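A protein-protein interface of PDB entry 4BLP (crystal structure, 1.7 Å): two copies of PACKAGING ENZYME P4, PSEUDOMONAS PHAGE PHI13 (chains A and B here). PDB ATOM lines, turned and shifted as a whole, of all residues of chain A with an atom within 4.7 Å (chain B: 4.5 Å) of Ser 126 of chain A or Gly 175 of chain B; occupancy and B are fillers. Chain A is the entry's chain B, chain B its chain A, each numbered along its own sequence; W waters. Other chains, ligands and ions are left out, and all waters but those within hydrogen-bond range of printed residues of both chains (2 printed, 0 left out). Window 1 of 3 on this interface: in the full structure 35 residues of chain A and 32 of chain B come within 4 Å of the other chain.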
ATOM      1  N   LEU A 124       4.307 -18.328  25.343  1.00  0.00           N
ATOM      2  CA  LEU A 124       3.343 -18.940  24.413  1.00  0.00           C
ATOM      3  C   LEU A 124       3.497 -20.470  24.434  1.00  0.00           C
ATOM      4  O   LEU A 124       3.532 -21.117  23.397  1.00  0.00           O
ATOM      5  CB  LEU A 124       3.531 -18.376  22.985  1.00  0.00           C
ATOM      6  CG  LEU A 124       3.532 -16.845  22.842  1.00  0.00           C
ATOM      7  CD1 LEU A 124       3.558 -16.453  21.384  1.00  0.00           C
ATOM      8  CD2 LEU A 124       2.328 -16.186  23.584  1.00  0.00           C
ATOM      9  N   LEU A 125       3.567 -21.024  25.636  1.00  0.00           N
ATOM     10  CA  LEU A 125       3.794 -22.443  25.823  1.00  0.00           C
ATOM     11  C   LEU A 125       2.536 -23.254  25.497  1.00  0.00           C
ATOM     12  O   LEU A 125       1.484 -23.099  26.146  1.00  0.00           O
ATOM     13  CB  LEU A 125       4.206 -22.708  27.283  1.00  0.00           C
ATOM     14  CG  LEU A 125       4.470 -24.170  27.654  1.00  0.00           C
ATOM     15  CD1 LEU A 125       5.644 -24.749  26.815  1.00  0.00           C
ATOM     16  CD2 LEU A 125       4.804 -24.239  29.130  1.00  0.00           C
ATOM     17  N   SER A 126       2.675 -24.081  24.510  1.00  0.00           N
ATOM     18  CA  SER A 126       1.666 -25.090  24.163  1.00  0.00           C
ATOM     19  C   SER A 126       2.254 -26.459  24.541  1.00  0.00           C
ATOM     20  O   SER A 126       3.206 -26.535  25.348  1.00  0.00           O
ATOM     21  CB  SER A 126       1.271 -25.000  22.679  1.00  0.00           C
ATOM     22  OG  SER A 126       0.192 -25.904  22.403  1.00  0.00           O
ATOM     23  N   VAL A 127       1.685 -27.553  23.996  1.00  0.00           N
ATOM     24  CA  VAL A 127       2.161 -28.913  24.265  1.00  0.00           C
ATOM     25  C   VAL A 127       2.467 -29.539  22.921  1.00  0.00           C
ATOM     26  O   VAL A 127       1.674 -29.377  22.004  1.00  0.00           O
ATOM     27  CB  VAL A 127       1.145 -29.761  25.073  1.00  0.00           C
ATOM     28  CG1 VAL A 127       1.627 -31.216  25.234  1.00  0.00           C
ATOM     29  CG2 VAL A 127       0.878 -29.105  26.446  1.00  0.00           C
ATOM     30  N   ARG A 128       3.621 -30.210  22.805  1.00  0.00           N
ATOM     31  CA  ARG A 128       4.058 -30.827  21.548  1.00  0.00           C
ATOM     32  C   ARG A 128       2.942 -31.678  20.920  1.00  0.00           C
ATOM     33  O   ARG A 128       2.447 -32.583  21.590  1.00  0.00           O
ATOM     34  CB  ARG A 128       5.284 -31.729  21.772  1.00  0.00           C
ATOM     35  CG  ARG A 128       6.529 -30.927  22.123  1.00  0.00           C
ATOM     36  CD  ARG A 128       7.716 -31.878  22.229  1.00  0.00           C
ATOM     37  NE  ARG A 128       8.944 -31.112  22.407  1.00  0.00           N
ATOM     38  CZ  ARG A 128      10.101 -31.629  22.804  1.00  0.00           C
ATOM     39  NH1 ARG A 128      10.204 -32.931  23.060  1.00  0.00           N
ATOM     40  NH2 ARG A 128      11.162 -30.850  22.965  1.00  0.00           N
ATOM     41  N   PRO A 129       2.529 -31.422  19.663  1.00  0.00           N
ATOM     42  CA  PRO A 129       1.494 -32.279  19.043  1.00  0.00           C
ATOM     43  C   PRO A 129       2.073 -33.653  18.703  1.00  0.00           C
ATOM     44  O   PRO A 129       3.178 -33.780  18.119  1.00  0.00           O
ATOM     45  CB  PRO A 129       1.094 -31.517  17.769  1.00  0.00           C
ATOM     46  CG  PRO A 129       1.680 -30.137  17.923  1.00  0.00           C
ATOM     47  CD  PRO A 129       2.912 -30.317  18.770  1.00  0.00           C
ATOM     48  N   THR A 240      -6.350 -27.278  23.502  1.00  0.00           N
ATOM     49  CA  THR A 240      -5.276 -27.925  22.721  1.00  0.00           C
ATOM     50  C   THR A 240      -4.206 -28.442  23.667  1.00  0.00           C
ATOM     51  O   THR A 240      -3.693 -29.527  23.446  1.00  0.00           O
ATOM     52  CB  THR A 240      -4.720 -26.980  21.661  1.00  0.00           C
ATOM     53  OG1 THR A 240      -5.806 -26.675  20.726  1.00  0.00           O
ATOM     54  CG2 THR A 240      -3.538 -27.607  20.891  1.00  0.00           C
ATOM     55  N   SER A 241      -3.850 -27.661  24.676  1.00  0.00           N
ATOM     56  CA  SER A 241      -2.822 -28.099  25.659  1.00  0.00           C
ATOM     57  C   SER A 241      -3.272 -29.396  26.357  1.00  0.00           C
ATOM     58  O   SER A 241      -2.493 -30.367  26.416  1.00  0.00           O
ATOM     59  CB  SER A 241      -2.563 -26.981  26.681  1.00  0.00           C
ATOM     60  OG  SER A 241      -1.942 -25.859  26.068  1.00  0.00           O
ATOM     61  N   ARG B 173       5.479 -28.468  14.037  1.00  0.00           N
ATOM     62  CA  ARG B 173       4.113 -28.552  14.529  1.00  0.00           C
ATOM     63  C   ARG B 173       4.038 -27.881  15.895  1.00  0.00           C
ATOM     64  O   ARG B 173       4.740 -28.274  16.832  1.00  0.00           O
ATOM     65  CB  ARG B 173       3.666 -30.030  14.546  1.00  0.00           C
ATOM     66  CG  ARG B 173       3.449 -30.544  13.080  1.00  0.00           C
ATOM     67  CD  ARG B 173       2.015 -30.274  12.620  1.00  0.00           C
ATOM     68  NE  ARG B 173       1.094 -31.087  13.417  1.00  0.00           N
ATOM     69  CZ  ARG B 173      -0.203 -30.856  13.618  1.00  0.00           C
ATOM     70  NH1 ARG B 173      -0.814 -29.864  12.992  1.00  0.00           N
ATOM     71  NH2 ARG B 173      -0.908 -31.657  14.393  1.00  0.00           N
ATOM     72  N   TRP B 174       3.217 -26.802  15.984  1.00  0.00           N
ATOM     73  CA  TRP B 174       3.160 -26.006  17.198  1.00  0.00           C
ATOM     74  C   TRP B 174       1.731 -25.553  17.468  1.00  0.00           C
ATOM     75  O   TRP B 174       1.110 -24.985  16.568  1.00  0.00           O
ATOM     76  CB  TRP B 174       4.079 -24.747  17.018  1.00  0.00           C
ATOM     77  CG  TRP B 174       4.147 -23.842  18.237  1.00  0.00           C
ATOM     78  CD1 TRP B 174       4.212 -24.233  19.539  1.00  0.00           C
ATOM     79  CD2 TRP B 174       4.168 -22.413  18.248  1.00  0.00           C
ATOM     80  NE1 TRP B 174       4.234 -23.129  20.368  1.00  0.00           N
ATOM     81  CE2 TRP B 174       4.192 -21.999  19.607  1.00  0.00           C
ATOM     82  CE3 TRP B 174       4.086 -21.430  17.254  1.00  0.00           C
ATOM     83  CZ2 TRP B 174       4.220 -20.649  19.996  1.00  0.00           C
ATOM     84  CZ3 TRP B 174       4.081 -20.073  17.647  1.00  0.00           C
ATOM     85  CH2 TRP B 174       4.167 -19.700  19.003  1.00  0.00           C
ATOM     86  N   GLY B 175       1.246 -25.763  18.684  1.00  0.00           N
ATOM     87  CA  GLY B 175      -0.042 -25.210  19.112  1.00  0.00           C
ATOM     88  C   GLY B 175      -1.281 -25.772  18.431  1.00  0.00           C
ATOM     89  O   GLY B 175      -2.361 -25.162  18.517  1.00  0.00           O
ATOM     90  N   GLU B 176      -1.146 -26.915  17.798  1.00  0.00           N
ATOM     91  CA  GLU B 176      -2.226 -27.620  17.084  1.00  0.00           C
ATOM     92  C   GLU B 176      -2.532 -28.966  17.728  1.00  0.00           C
ATOM     93  O   GLU B 176      -1.624 -29.578  18.305  1.00  0.00           O
ATOM     94  CB  GLU B 176      -1.779 -27.859  15.639  1.00  0.00           C
ATOM     95  CG  GLU B 176      -1.641 -26.559  14.861  1.00  0.00           C
ATOM     96  CD  GLU B 176      -2.947 -25.925  14.429  1.00  0.00           C
ATOM     97  OE1 GLU B 176      -4.018 -26.552  14.581  1.00  0.00           O
ATOM     98  OE2 GLU B 176      -2.914 -24.755  14.005  1.00  0.00           O
ATOM     99  N   ALA B 191       7.071 -27.000  21.620  1.00  0.00           N
ATOM    100  CA  ALA B 191       6.130 -26.583  22.654  1.00  0.00           C
ATOM    101  C   ALA B 191       5.957 -25.060  22.761  1.00  0.00           C
ATOM    102  O   ALA B 191       4.821 -24.606  22.777  1.00  0.00           O
ATOM    103  CB  ALA B 191       6.580 -27.138  24.006  1.00  0.00           C
ATOM    104  N   ARG B 216      -0.993 -20.312  15.521  1.00  0.00           N
ATOM    105  CA  ARG B 216      -2.193 -20.206  16.370  1.00  0.00           C
ATOM    106  C   ARG B 216      -1.882 -19.605  17.745  1.00  0.00           C
ATOM    107  O   ARG B 216      -2.586 -18.700  18.202  1.00  0.00           O
ATOM    108  CB  ARG B 216      -2.686 -21.630  16.569  1.00  0.00           C
ATOM    109  CG  ARG B 216      -4.120 -21.701  16.787  1.00  0.00           C
ATOM    110  CD  ARG B 216      -4.510 -23.135  16.558  1.00  0.00           C
ATOM    111  NE  ARG B 216      -5.852 -23.269  17.073  1.00  0.00           N
ATOM    112  CZ  ARG B 216      -6.180 -24.064  18.071  1.00  0.00           C
ATOM    113  NH1 ARG B 216      -5.271 -24.865  18.620  1.00  0.00           N
ATOM    114  NH2 ARG B 216      -7.420 -24.100  18.505  1.00  0.00           N
ATOM    115  N   ASN B 217      -0.786 -20.083  18.407  1.00  0.00           N
ATOM    116  CA  ASN B 217      -0.461 -19.539  19.730  1.00  0.00           C
ATOM    117  C   ASN B 217       0.005 -18.087  19.698  1.00  0.00           C
ATOM    118  O   ASN B 217      -0.082 -17.398  20.719  1.00  0.00           O
ATOM    119  CB  ASN B 217       0.589 -20.393  20.427  1.00  0.00           C
ATOM    120  CG  ASN B 217      -0.032 -21.263  21.469  1.00  0.00           C
ATOM    121  OD1 ASN B 217      -1.264 -21.487  21.490  1.00  0.00           O
ATOM    122  ND2 ASN B 217       0.764 -21.627  22.450  1.00  0.00           N
HETATM  123  O   HOH W   1      -0.930 -22.458  25.059  1.00  0.00           O
HETATM  124  O   HOH W   2       2.685 -27.155  20.526  1.00  0.00           O
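No position is printed for both chains.
Of the 14 pairs that touch across the chains among the printed residues, none has its exchanged pair printed and touching as well.
Printed residues of chain A that touch a printed residue of chain B: Leu 124, Leu 125, Ser 126, Arg 128, Pro 129 and Thr 240.
Among the printed residues, 14 pairs touch across the chains.
Among the printed residues, merely in contact across the chains: Pro 129 of chain A with Arg 173 of chain B (3.4 Å), Ser 126 of chain A with Gly 175 of chain B (3.4 Å), Pro 129 of chain A with Glu 176 of chain B (3.4 Å), Ser 126 of chain A with Asn 217 of chain B (3.4 Å), Leu 124 of chain A with Trp 174 of chain B (3.5 Å), Thr 240 of chain A with Glu 176 of chain B (3.6 Å), Thr 240 of chain A with Gly 175 of chain B (3.6 Å), Leu 124 of chain A with Ala 191 of chain B (3.8 Å), Leu 125 of chain A with Ala 191 of chain B (3.8 Å), Leu 125 of chain A with Asn 217 of chain B (3.9 Å) and Arg 128 of chain A with Ala 191 of chain B (3.996 Å).
Water W2 lies within hydrogen-bond range of the backbone NH of Gly 175 of chain B (2.7 Å), the backbone carbonyl oxygen of Val 127 of chain A (2.9 Å) and the side-chain hydroxyl of Ser 126 of chain A (3.4 Å).
Water W1 bridges the backbone carbonyl oxygen of Leu 125 of chain A (2.7 Å) and the side-chain amide nitrogen of Asn 217 of chain B (3.2 Å).
The backbone NH of Ser 126 of chain A sits at hydrogen-bond distance from the backbone carbonyl oxygen of Ala 191 of chain B, 2.8 Å away.
The guanidinium group (NH1) of Arg 216 of chain B sits at hydrogen-bond distance from the side-chain hydroxyl (OG1) of Thr 240 of chain A, 2.8 Å away.
ND2 of Asn 217 of chain B sits at hydrogen-bond distance from O of Leu 124 of chain A, 3.0 Å away.
O of Gly 175 of chain B is in hydrogen-bond range of NH1 of Arg 216 of chain B, at 2.9 Å.
The backbone carbonyl oxygen (O) of Ala 191 of chain B is in hydrogen-bond range of the indole nitrogen (NE1) of Trp 174 of chain B (2.9 Å).
Of chain B, only Gly 175, Ala 191 and Asn 217 come within 4 Å of Ser 126 of chain A.
Gly 175 of chain B touches just these residues of chain A: Ser 126 and Thr 240.
Printed residues of chain B within 4 Å of Leu 125 of chain A: Ala 191 (3.8 Å) and Asn 217 (3.9 Å).
Of the printed residues of chain A, Trp 174 of chain B touches Leu 124 (3.5 Å).
Of the printed residues of chain B, Pro 129 of chain A touches Arg 173 and Glu 176.
Of the printed residues of chain A, Glu 176 of chain B touches Pro 129 (3.4 Å) and Thr 240 (3.6 Å).
Val 127 of chain A touches none of the printed residues of chain B.
The nearest residue of chain B that does not touch Ser 126 of chain A is Trp 174 of chain B (4.2 Å).
The nearest residue of chain A that does not touch Gly 175 of chain B is Pro 129 of chain A (4.5 Å).
The nearest printed residue of chain B that does not touch Leu 125 of chain A is Trp 174 of chain B (5.4 Å).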
